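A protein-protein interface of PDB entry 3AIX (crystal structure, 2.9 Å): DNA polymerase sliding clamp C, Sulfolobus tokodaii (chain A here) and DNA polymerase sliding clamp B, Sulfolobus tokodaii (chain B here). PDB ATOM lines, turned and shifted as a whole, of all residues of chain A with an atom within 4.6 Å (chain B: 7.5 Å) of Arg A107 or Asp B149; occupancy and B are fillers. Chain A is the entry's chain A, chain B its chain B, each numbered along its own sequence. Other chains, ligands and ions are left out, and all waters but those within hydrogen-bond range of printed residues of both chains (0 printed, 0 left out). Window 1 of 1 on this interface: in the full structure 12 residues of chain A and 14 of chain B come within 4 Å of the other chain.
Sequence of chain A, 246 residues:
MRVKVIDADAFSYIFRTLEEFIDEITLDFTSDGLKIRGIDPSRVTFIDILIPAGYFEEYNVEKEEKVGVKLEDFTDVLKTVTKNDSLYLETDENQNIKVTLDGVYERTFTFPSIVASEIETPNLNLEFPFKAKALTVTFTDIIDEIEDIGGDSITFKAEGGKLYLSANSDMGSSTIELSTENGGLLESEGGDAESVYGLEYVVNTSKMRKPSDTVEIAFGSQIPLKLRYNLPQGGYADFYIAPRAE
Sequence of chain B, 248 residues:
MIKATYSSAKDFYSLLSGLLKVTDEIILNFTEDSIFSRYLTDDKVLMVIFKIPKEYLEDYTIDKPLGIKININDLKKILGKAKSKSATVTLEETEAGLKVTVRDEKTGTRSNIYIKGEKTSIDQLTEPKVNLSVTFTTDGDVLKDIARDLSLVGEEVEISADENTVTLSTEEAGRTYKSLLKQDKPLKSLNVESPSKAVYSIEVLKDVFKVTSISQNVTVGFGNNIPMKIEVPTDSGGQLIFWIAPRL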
ATOM      1  N   THR A  80       0.923 -16.084  27.732  1.00  0.00           N
ATOM      2  CA  THR A  80       0.711 -14.940  28.612  1.00  0.00           C
ATOM      3  C   THR A  80      -0.720 -14.896  29.130  1.00  0.00           C
ATOM      4  O   THR A  80      -1.204 -13.843  29.546  1.00  0.00           O
ATOM      5  CB  THR A  80       1.012 -13.613  27.893  1.00  0.00           C
ATOM      6  OG1 THR A  80      -0.016 -13.341  26.933  1.00  0.00           O
ATOM      7  CG2 THR A  80       2.357 -13.677  27.190  1.00  0.00           C
ATOM      8  N   ASP A  85      -8.407 -15.035  31.980  1.00  0.00           N
ATOM      9  CA  ASP A  85      -8.389 -14.393  30.670  1.00  0.00           C
ATOM     10  C   ASP A  85      -9.338 -15.051  29.679  1.00  0.00           C
ATOM     11  O   ASP A  85      -9.420 -16.277  29.598  1.00  0.00           O
ATOM     12  CB  ASP A  85      -6.972 -14.392  30.092  1.00  0.00           C
ATOM     13  CG  ASP A  85      -6.114 -13.283  30.658  1.00  0.00           C
ATOM     14  OD1 ASP A  85      -6.657 -12.194  30.942  1.00  0.00           O
ATOM     15  OD2 ASP A  85      -4.892 -13.499  30.809  1.00  0.00           O
ATOM     16  N   VAL A  99      -5.372 -11.857  17.783  1.00  0.00           N
ATOM     17  CA  VAL A  99      -5.616 -12.528  19.051  1.00  0.00           C
ATOM     18  C   VAL A  99      -5.800 -11.492  20.151  1.00  0.00           C
ATOM     19  O   VAL A  99      -4.904 -10.692  20.417  1.00  0.00           O
ATOM     20  CB  VAL A  99      -4.460 -13.469  19.420  1.00  0.00           C
ATOM     21  CG1 VAL A  99      -4.744 -14.164  20.740  1.00  0.00           C
ATOM     22  CG2 VAL A  99      -4.240 -14.485  18.317  1.00  0.00           C
ATOM     23  N   THR A 100      -6.967 -11.505  20.785  1.00  0.00           N
ATOM     24  CA  THR A 100      -7.274 -10.537  21.830  1.00  0.00           C
ATOM     25  C   THR A 100      -7.517 -11.207  23.177  1.00  0.00           C
ATOM     26  O   THR A 100      -8.506 -11.913  23.361  1.00  0.00           O
ATOM     27  CB  THR A 100      -8.508  -9.695  21.464  1.00  0.00           C
ATOM     28  OG1 THR A 100      -8.243  -8.952  20.269  1.00  0.00           O
ATOM     29  CG2 THR A 100      -8.846  -8.732  22.591  1.00  0.00           C
ATOM     30  N   LEU A 101      -6.607 -10.978  24.117  1.00  0.00           N
ATOM     31  CA  LEU A 101      -6.770 -11.482  25.474  1.00  0.00           C
ATOM     32  C   LEU A 101      -7.422 -10.411  26.338  1.00  0.00           C
ATOM     33  O   LEU A 101      -7.061  -9.237  26.255  1.00  0.00           O
ATOM     34  CB  LEU A 101      -5.417 -11.885  26.062  1.00  0.00           C
ATOM     35  CG  LEU A 101      -4.545 -12.780  25.179  1.00  0.00           C
ATOM     36  CD1 LEU A 101      -3.300 -13.227  25.928  1.00  0.00           C
ATOM     37  CD2 LEU A 101      -5.333 -13.983  24.681  1.00  0.00           C
ATOM     38  N   GLY A 103      -8.654  -9.780  30.403  1.00  0.00           N
ATOM     39  CA  GLY A 103      -8.803 -10.150  31.798  1.00  0.00           C
ATOM     40  C   GLY A 103      -8.644  -8.929  32.680  1.00  0.00           C
ATOM     41  O   GLY A 103      -9.562  -8.116  32.799  1.00  0.00           O
ATOM     42  N   TYR A 105      -6.620  -6.551  31.958  1.00  0.00           N
ATOM     43  CA  TYR A 105      -6.656  -5.505  30.943  1.00  0.00           C
ATOM     44  C   TYR A 105      -6.852  -6.118  29.561  1.00  0.00           C
ATOM     45  O   TYR A 105      -6.703  -7.327  29.383  1.00  0.00           O
ATOM     46  CB  TYR A 105      -5.382  -4.659  30.981  1.00  0.00           C
ATOM     47  CG  TYR A 105      -4.120  -5.413  30.622  1.00  0.00           C
ATOM     48  CD1 TYR A 105      -3.617  -6.401  31.457  1.00  0.00           C
ATOM     49  CD2 TYR A 105      -3.426  -5.126  29.456  1.00  0.00           C
ATOM     50  CE1 TYR A 105      -2.463  -7.089  31.135  1.00  0.00           C
ATOM     51  CE2 TYR A 105      -2.271  -5.808  29.125  1.00  0.00           C
ATOM     52  CZ  TYR A 105      -1.794  -6.788  29.970  1.00  0.00           C
ATOM     53  OH  TYR A 105      -0.642  -7.471  29.648  1.00  0.00           O
ATOM     54  N   GLU A 106      -7.193  -5.281  28.587  1.00  0.00           N
ATOM     55  CA  GLU A 106      -7.418  -5.752  27.227  1.00  0.00           C
ATOM     56  C   GLU A 106      -6.183  -5.524  26.364  1.00  0.00           C
ATOM     57  O   GLU A 106      -5.633  -4.425  26.325  1.00  0.00           O
ATOM     58  CB  GLU A 106      -8.629  -5.052  26.612  1.00  0.00           C
ATOM     59  CG  GLU A 106      -8.965  -5.513  25.205  1.00  0.00           C
ATOM     60  CD  GLU A 106     -10.096  -4.717  24.589  1.00  0.00           C
ATOM     61  OE1 GLU A 106     -10.749  -3.947  25.325  1.00  0.00           O
ATOM     62  OE2 GLU A 106     -10.331  -4.856  23.370  1.00  0.00           O
ATOM     63  N   ARG A 107      -5.753  -6.571  25.671  1.00  0.00           N
ATOM     64  CA  ARG A 107      -4.565  -6.500  24.830  1.00  0.00           C
ATOM     65  C   ARG A 107      -4.772  -7.307  23.557  1.00  0.00           C
ATOM     66  O   ARG A 107      -5.388  -8.372  23.582  1.00  0.00           O
ATOM     67  CB  ARG A 107      -3.353  -7.025  25.597  1.00  0.00           C
ATOM     68  CG  ARG A 107      -3.567  -8.397  26.204  1.00  0.00           C
ATOM     69  CD  ARG A 107      -2.497  -8.714  27.227  1.00  0.00           C
ATOM     70  NE  ARG A 107      -2.721  -9.999  27.880  1.00  0.00           N
ATOM     71  CZ  ARG A 107      -3.667 -10.219  28.787  1.00  0.00           C
ATOM     72  NH1 ARG A 107      -3.796 -11.418  29.335  1.00  0.00           N
ATOM     73  NH2 ARG A 107      -4.490  -9.242  29.141  1.00  0.00           N
ATOM     74  N   THR A 108      -4.257  -6.799  22.443  1.00  0.00           N
ATOM     75  CA  THR A 108      -4.449  -7.453  21.155  1.00  0.00           C
ATOM     76  C   THR A 108      -3.139  -7.654  20.406  1.00  0.00           C
ATOM     77  O   THR A 108      -2.357  -6.720  20.238  1.00  0.00           O
ATOM     78  CB  THR A 108      -5.415  -6.657  20.264  1.00  0.00           C
ATOM     79  OG1 THR A 108      -6.687  -6.548  20.915  1.00  0.00           O
ATOM     80  CG2 THR A 108      -5.594  -7.350  18.922  1.00  0.00           C
ATOM     81  N   PHE A 109      -2.907  -8.885  19.962  1.00  0.00           N
ATOM     82  CA  PHE A 109      -1.743  -9.209  19.149  1.00  0.00           C
ATOM     83  C   PHE A 109      -2.170  -9.523  17.721  1.00  0.00           C
ATOM     84  O   PHE A 109      -3.186 -10.180  17.498  1.00  0.00           O
ATOM     85  CB  PHE A 109      -0.989 -10.399  19.740  1.00  0.00           C
ATOM     86  CG  PHE A 109      -0.359 -10.119  21.073  1.00  0.00           C
ATOM     87  CD1 PHE A 109      -1.103 -10.209  22.238  1.00  0.00           C
ATOM     88  CD2 PHE A 109       0.981  -9.775  21.162  1.00  0.00           C
ATOM     89  CE1 PHE A 109      -0.524  -9.957  23.467  1.00  0.00           C
ATOM     90  CE2 PHE A 109       1.564  -9.523  22.387  1.00  0.00           C
ATOM     91  CZ  PHE A 109       0.811  -9.614  23.542  1.00  0.00           C
ATOM     92  N   VAL B 142       0.613  -4.907  36.641  1.00  0.00           N
ATOM     93  CA  VAL B 142       0.064  -4.678  35.311  1.00  0.00           C
ATOM     94  C   VAL B 142       1.150  -4.193  34.360  1.00  0.00           C
ATOM     95  O   VAL B 142       1.292  -4.707  33.250  1.00  0.00           O
ATOM     96  CB  VAL B 142      -1.068  -3.639  35.339  1.00  0.00           C
ATOM     97  CG1 VAL B 142      -1.545  -3.341  33.926  1.00  0.00           C
ATOM     98  CG2 VAL B 142      -2.215  -4.128  36.209  1.00  0.00           C
ATOM     99  N   LEU B 143       1.913  -3.200  34.802  1.00  0.00           N
ATOM    100  CA  LEU B 143       2.986  -2.644  33.989  1.00  0.00           C
ATOM    101  C   LEU B 143       4.031  -3.705  33.662  1.00  0.00           C
ATOM    102  O   LEU B 143       4.627  -3.689  32.587  1.00  0.00           O
ATOM    103  CB  LEU B 143       3.634  -1.455  34.697  1.00  0.00           C
ATOM    104  CG  LEU B 143       2.711  -0.275  35.011  1.00  0.00           C
ATOM    105  CD1 LEU B 143       3.479   0.833  35.708  1.00  0.00           C
ATOM    106  CD2 LEU B 143       2.053   0.248  33.746  1.00  0.00           C
ATOM    107  N   LYS B 144       4.248  -4.629  34.593  1.00  0.00           N
ATOM    108  CA  LYS B 144       5.207  -5.705  34.377  1.00  0.00           C
ATOM    109  C   LYS B 144       4.690  -6.695  33.337  1.00  0.00           C
ATOM    110  O   LYS B 144       5.461  -7.229  32.540  1.00  0.00           O
ATOM    111  CB  LYS B 144       5.520  -6.427  35.688  1.00  0.00           C
ATOM    112  CG  LYS B 144       6.577  -7.513  35.551  1.00  0.00           C
ATOM    113  CD  LYS B 144       6.922  -8.129  36.896  1.00  0.00           C
ATOM    114  CE  LYS B 144       8.037  -9.154  36.760  1.00  0.00           C
ATOM    115  NZ  LYS B 144       8.422  -9.736  38.077  1.00  0.00           N
ATOM    116  N   ASP B 145       3.384  -6.938  33.351  1.00  0.00           N
ATOM    117  CA  ASP B 145       2.761  -7.799  32.355  1.00  0.00           C
ATOM    118  C   ASP B 145       2.889  -7.173  30.972  1.00  0.00           C
ATOM    119  O   ASP B 145       3.243  -7.847  30.004  1.00  0.00           O
ATOM    120  CB  ASP B 145       1.287  -8.038  32.690  1.00  0.00           C
ATOM    121  CG  ASP B 145       1.100  -8.932  33.900  1.00  0.00           C
ATOM    122  OD1 ASP B 145       2.082  -9.582  34.320  1.00  0.00           O
ATOM    123  OD2 ASP B 145      -0.030  -8.989  34.430  1.00  0.00           O
ATOM    124  N   ILE B 146       2.602  -5.879  30.887  1.00  0.00           N
ATOM    125  CA  ILE B 146       2.728  -5.152  29.631  1.00  0.00           C
ATOM    126  C   ILE B 146       4.178  -5.138  29.160  1.00  0.00           C
ATOM    127  O   ILE B 146       4.449  -5.131  27.960  1.00  0.00           O
ATOM    128  CB  ILE B 146       2.200  -3.712  29.755  1.00  0.00           C
ATOM    129  CG1 ILE B 146       0.731  -3.725  30.179  1.00  0.00           C
ATOM    130  CG2 ILE B 146       2.363  -2.968  28.441  1.00  0.00           C
ATOM    131  CD1 ILE B 146       0.095  -2.355  30.227  1.00  0.00           C
ATOM    132  N   ALA B 147       5.109  -5.141  30.108  1.00  0.00           N
ATOM    133  CA  ALA B 147       6.525  -5.237  29.775  1.00  0.00           C
ATOM    134  C   ALA B 147       6.793  -6.562  29.071  1.00  0.00           C
ATOM    135  O   ALA B 147       7.475  -6.611  28.047  1.00  0.00           O
ATOM    136  CB  ALA B 147       7.375  -5.116  31.026  1.00  0.00           C
ATOM    137  N   ARG B 148       6.244  -7.635  29.629  1.00  0.00           N
ATOM    138  CA  ARG B 148       6.344  -8.956  29.024  1.00  0.00           C
ATOM    139  C   ARG B 148       5.742  -8.955  27.620  1.00  0.00           C
ATOM    140  O   ARG B 148       6.295  -9.558  26.700  1.00  0.00           O
ATOM    141  CB  ARG B 148       5.634  -9.987  29.899  1.00  0.00           C
ATOM    142  CG  ARG B 148       5.380 -11.319  29.221  1.00  0.00           C
ATOM    143  CD  ARG B 148       4.147 -11.979  29.811  1.00  0.00           C
ATOM    144  NE  ARG B 148       2.978 -11.109  29.706  1.00  0.00           N
ATOM    145  CZ  ARG B 148       1.825 -11.324  30.331  1.00  0.00           C
ATOM    146  NH1 ARG B 148       1.679 -12.387  31.115  1.00  0.00           N
ATOM    147  NH2 ARG B 148       0.817 -10.475  30.175  1.00  0.00           N
ATOM    148  N   ASP B 149       4.610  -8.277  27.465  1.00  0.00           N
ATOM    149  CA  ASP B 149       3.966  -8.150  26.162  1.00  0.00           C
ATOM    150  C   ASP B 149       4.906  -7.498  25.155  1.00  0.00           C
ATOM    151  O   ASP B 149       5.144  -8.033  24.072  1.00  0.00           O
ATOM    152  CB  ASP B 149       2.684  -7.322  26.272  1.00  0.00           C
ATOM    153  CG  ASP B 149       1.625  -7.990  27.124  1.00  0.00           C
ATOM    154  OD1 ASP B 149       1.851  -9.135  27.571  1.00  0.00           O
ATOM    155  OD2 ASP B 149       0.564  -7.368  27.346  1.00  0.00           O
ATOM    156  N   LEU B 150       5.437  -6.337  25.525  1.00  0.00           N
ATOM    157  CA  LEU B 150       6.325  -5.578  24.652  1.00  0.00           C
ATOM    158  C   LEU B 150       7.580  -6.369  24.296  1.00  0.00           C
ATOM    159  O   LEU B 150       8.234  -6.094  23.290  1.00  0.00           O
ATOM    160  CB  LEU B 150       6.708  -4.252  25.313  1.00  0.00           C
ATOM    161  CG  LEU B 150       5.570  -3.284  25.642  1.00  0.00           C
ATOM    162  CD1 LEU B 150       6.104  -2.068  26.384  1.00  0.00           C
ATOM    163  CD2 LEU B 150       4.823  -2.862  24.384  1.00  0.00           C
ATOM    164  N   SER B 151       7.912  -7.351  25.126  1.00  0.00           N
ATOM    165  CA  SER B 151       9.083  -8.187  24.896  1.00  0.00           C
ATOM    166  C   SER B 151       8.930  -9.044  23.641  1.00  0.00           C
ATOM    167  O   SER B 151       9.918  -9.475  23.049  1.00  0.00           O
ATOM    168  CB  SER B 151       9.343  -9.084  26.109  1.00  0.00           C
ATOM    169  OG  SER B 151      10.265 -10.114  25.797  1.00  0.00           O
ATOM    170  N   LEU B 152       7.686  -9.285  23.239  1.00  0.00           N
ATOM    171  CA  LEU B 152       7.406 -10.177  22.119  1.00  0.00           C
ATOM    172  C   LEU B 152       7.415  -9.451  20.779  1.00  0.00           C
ATOM    173  O   LEU B 152       7.684 -10.056  19.741  1.00  0.00           O
ATOM    174  CB  LEU B 152       6.061 -10.876  22.320  1.00  0.00           C
ATOM    175  CG  LEU B 152       5.930 -11.733  23.578  1.00  0.00           C
ATOM    176  CD1 LEU B 152       4.508 -12.247  23.729  1.00  0.00           C
ATOM    177  CD2 LEU B 152       6.924 -12.884  23.547  1.00  0.00           C
ATOM    178  N   VAL B 153       7.119  -8.157  20.805  1.00  0.00           N
ATOM    179  CA  VAL B 153       7.028  -7.377  19.576  1.00  0.00           C
ATOM    180  C   VAL B 153       7.192  -5.883  19.832  1.00  0.00           C
ATOM    181  O   VAL B 153       6.736  -5.364  20.852  1.00  0.00           O
ATOM    182  CB  VAL B 153       5.681  -7.620  18.862  1.00  0.00           C
ATOM    183  CG1 VAL B 153       4.524  -7.462  19.836  1.00  0.00           C
ATOM    184  CG2 VAL B 153       5.525  -6.681  17.676  1.00  0.00           C
ATOM    185  N   GLY B 154       7.851  -5.197  18.904  1.00  0.00           N
ATOM    186  CA  GLY B 154       7.966  -3.753  18.974  1.00  0.00           C
ATOM    187  C   GLY B 154       9.386  -3.230  19.062  1.00  0.00           C
ATOM    188  O   GLY B 154      10.252  -3.837  19.693  1.00  0.00           O
ATOM    189  N   THR B 170       2.677  -0.978  19.461  1.00  0.00           N
ATOM    190  CA  THR B 170       3.976  -1.236  18.847  1.00  0.00           C
ATOM    191  C   THR B 170       3.810  -2.026  17.554  1.00  0.00           C
ATOM    192  O   THR B 170       2.797  -2.700  17.353  1.00  0.00           O
ATOM    193  CB  THR B 170       4.915  -2.021  19.782  1.00  0.00           C
ATOM    194  OG1 THR B 170       4.413  -3.350  19.962  1.00  0.00           O
ATOM    195  CG2 THR B 170       5.031  -1.334  21.134  1.00  0.00           C
ATOM    196  N   TYR B 177       1.052  -5.028  18.348  1.00  0.00           N
ATOM    197  CA  TYR B 177       0.558  -5.104  19.716  1.00  0.00           C
ATOM    198  C   TYR B 177      -0.192  -3.827  20.075  1.00  0.00           C
ATOM    199  O   TYR B 177       0.158  -2.740  19.613  1.00  0.00           O
ATOM    200  CB  TYR B 177       1.709  -5.345  20.694  1.00  0.00           C
ATOM    201  CG  TYR B 177       1.314  -5.230  22.148  1.00  0.00           C
ATOM    202  CD1 TYR B 177       0.649  -6.266  22.794  1.00  0.00           C
ATOM    203  CD2 TYR B 177       1.612  -4.088  22.879  1.00  0.00           C
ATOM    204  CE1 TYR B 177       0.289  -6.164  24.124  1.00  0.00           C
ATOM    205  CE2 TYR B 177       1.256  -3.977  24.209  1.00  0.00           C
ATOM    206  CZ  TYR B 177       0.597  -5.016  24.827  1.00  0.00           C
ATOM    207  OH  TYR B 177       0.244  -4.906  26.152  1.00  0.00           O
ATOM    208  N   LYS B 178      -1.224  -3.963  20.898  1.00  0.00           N
ATOM    209  CA  LYS B 178      -2.054  -2.825  21.269  1.00  0.00           C
ATOM    210  C   LYS B 178      -2.895  -3.159  22.494  1.00  0.00           C
ATOM    211  O   LYS B 178      -3.854  -3.924  22.405  1.00  0.00           O
ATOM    212  CB  LYS B 178      -2.962  -2.442  20.099  1.00  0.00           C
ATOM    213  CG  LYS B 178      -3.678  -1.112  20.253  1.00  0.00           C
ATOM    214  CD  LYS B 178      -4.583  -0.850  19.055  1.00  0.00           C
ATOM    215  CE  LYS B 178      -5.160   0.558  19.071  1.00  0.00           C
ATOM    216  NZ  LYS B 178      -4.119   1.594  18.815  1.00  0.00           N
ATOM    217  N   SER B 179      -2.529  -2.593  23.642  1.00  0.00           N
ATOM    218  CA  SER B 179      -3.295  -2.811  24.864  1.00  0.00           C
ATOM    219  C   SER B 179      -4.087  -1.565  25.246  1.00  0.00           C
ATOM    220  O   SER B 179      -3.733  -0.452  24.863  1.00  0.00           O
ATOM    221  CB  SER B 179      -2.389  -3.252  26.018  1.00  0.00           C
ATOM    222  OG  SER B 179      -1.397  -2.283  26.294  1.00  0.00           O
ATOM    223  N   LEU B 180      -5.164  -1.764  25.998  1.00  0.00           N
ATOM    224  CA  LEU B 180      -6.039  -0.665  26.388  1.00  0.00           C
ATOM    225  C   LEU B 180      -6.212  -0.602  27.900  1.00  0.00           C
ATOM    226  O   LEU B 180      -6.699  -1.547  28.521  1.00  0.00           O
ATOM    227  CB  LEU B 180      -7.408  -0.812  25.723  1.00  0.00           C
ATOM    228  CG  LEU B 180      -7.438  -0.851  24.196  1.00  0.00           C
ATOM    229  CD1 LEU B 180      -8.836  -1.190  23.709  1.00  0.00           C
ATOM    230  CD2 LEU B 180      -6.964   0.472  23.611  1.00  0.00           C
ATOM    231  N   ILE B 202      11.222   1.145  23.713  1.00  0.00           N
ATOM    232  CA  ILE B 202      10.627  -0.065  24.258  1.00  0.00           C
ATOM    233  C   ILE B 202      11.598  -0.764  25.207  1.00  0.00           C
ATOM    234  O   ILE B 202      11.184  -1.403  26.172  1.00  0.00           O
ATOM    235  CB  ILE B 202      10.198  -1.033  23.138  1.00  0.00           C
ATOM    236  CG1 ILE B 202       9.352  -2.174  23.705  1.00  0.00           C
ATOM    237  CG2 ILE B 202      11.415  -1.566  22.393  1.00  0.00           C
ATOM    238  CD1 ILE B 202       8.713  -3.037  22.643  1.00  0.00           C
ATOM    239  N   LYS B 206      10.524  -1.150  29.049  1.00  0.00           N
ATOM    240  CA  LYS B 206      10.463  -2.508  29.576  1.00  0.00           C
ATOM    241  C   LYS B 206      11.184  -2.622  30.913  1.00  0.00           C
ATOM    242  O   LYS B 206      10.612  -3.079  31.901  1.00  0.00           O
ATOM    243  CB  LYS B 206      11.077  -3.493  28.581  1.00  0.00           C
ATOM    244  CG  LYS B 206      10.147  -3.914  27.457  1.00  0.00           C
ATOM    245  CD  LYS B 206      10.934  -4.411  26.254  1.00  0.00           C
ATOM    246  CE  LYS B 206      11.970  -5.450  26.651  1.00  0.00           C
ATOM    247  NZ  LYS B 206      12.838  -5.825  25.499  1.00  0.00           N
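Hydrophobic or aromatic side chains of chain B that line the printed part of chain A: Ile B146, Tyr B177 and Leu B180.
Printed residues of chain A that touch a printed residue of chain B: Thr A80, Tyr A105, Glu A106, Arg A107, Thr A108 and Phe A109.
Among the printed residues, 14 pairs touch across the chains.
Among the printed residues, no Asp or Glu carboxylate lies within 4 Å of a Lys or Arg side-chain nitrogen of the other chain.
The backbone carbonyl oxygen of Glu A106 lies within hydrogen-bond range of the backbone NH of Leu B180, at 2.7 Å.
The side-chain hydroxyl (OH) of Tyr A105 is in hydrogen-bond range of the guanidinium group (NH2) of Arg B148, at 3.4 Å.
The side-chain carboxylate of Asp B149 lies within hydrogen-bond range of the side-chain hydroxyl of Tyr A105, at 2.6 Å.
The backbone NH of Thr A108 is in hydrogen-bond range of the backbone carbonyl oxygen of Lys B178 (2.9 Å).
Among the printed residues, merely in contact across the chains: Thr A80 with Arg B148 (3.4 Å), Tyr A105 with Asp B145 (3.6 Å), Tyr A105 with Ile B146 (3.8 Å), Tyr A105 with Tyr B177 (3.997 Å), Glu A106 with Ser B179 (3.2 Å), Arg A107 with Asp B149 (3.3 Å), Arg A107 with Lys B178 (3.6 Å), Arg A107 with Ser B179 (3.9 Å), Thr A108 with Tyr B177 (3.4 Å) and Phe A109 with Tyr B177 (3.4 Å).
Of chain B, only Asp B149, Lys B178 and Ser B179 come within 4 Å of Arg A107.
Printed residues of chain A within 4 Å of Asp B149: Tyr A105 (2.6 Å) and Arg A107 (3.3 Å).
Of the printed residues of chain B, Glu A106 touches Ser B179 (3.2 Å) and Leu B180 (2.7 Å).
Printed residues of chain A within 4 Å of Leu B180: Glu A106 (2.7 Å).
The nearest printed residue of chain A that does not touch Asp B149 is Phe A109 (4.02 Å).
The nearest printed residue of chain B that does not touch Thr A80 is Leu B152 (4.3 Å).
O of Asp B145 sits close to NE of Arg B148 (3.3 Å).
OG1 of Thr A100 sits at hydrogen-bond distance from OG1 of Thr A108.
NH2 of Arg B148 is in salt-bridge range of OD1 of Asp B149 (3.1 Å).
The backbone carbonyl oxygen (O) of Arg A107 is in hydrogen-bond range of the backbone NH (N) of Leu A101, 2.9 Å away.
The backbone carbonyl oxygen (O) of Thr B170 is in hydrogen-bond range of the backbone NH (N) of Tyr B177, 3.1 Å away.
O of Tyr A105 lies within hydrogen-bond range of NH2 of Arg A107, at 2.9 Å.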
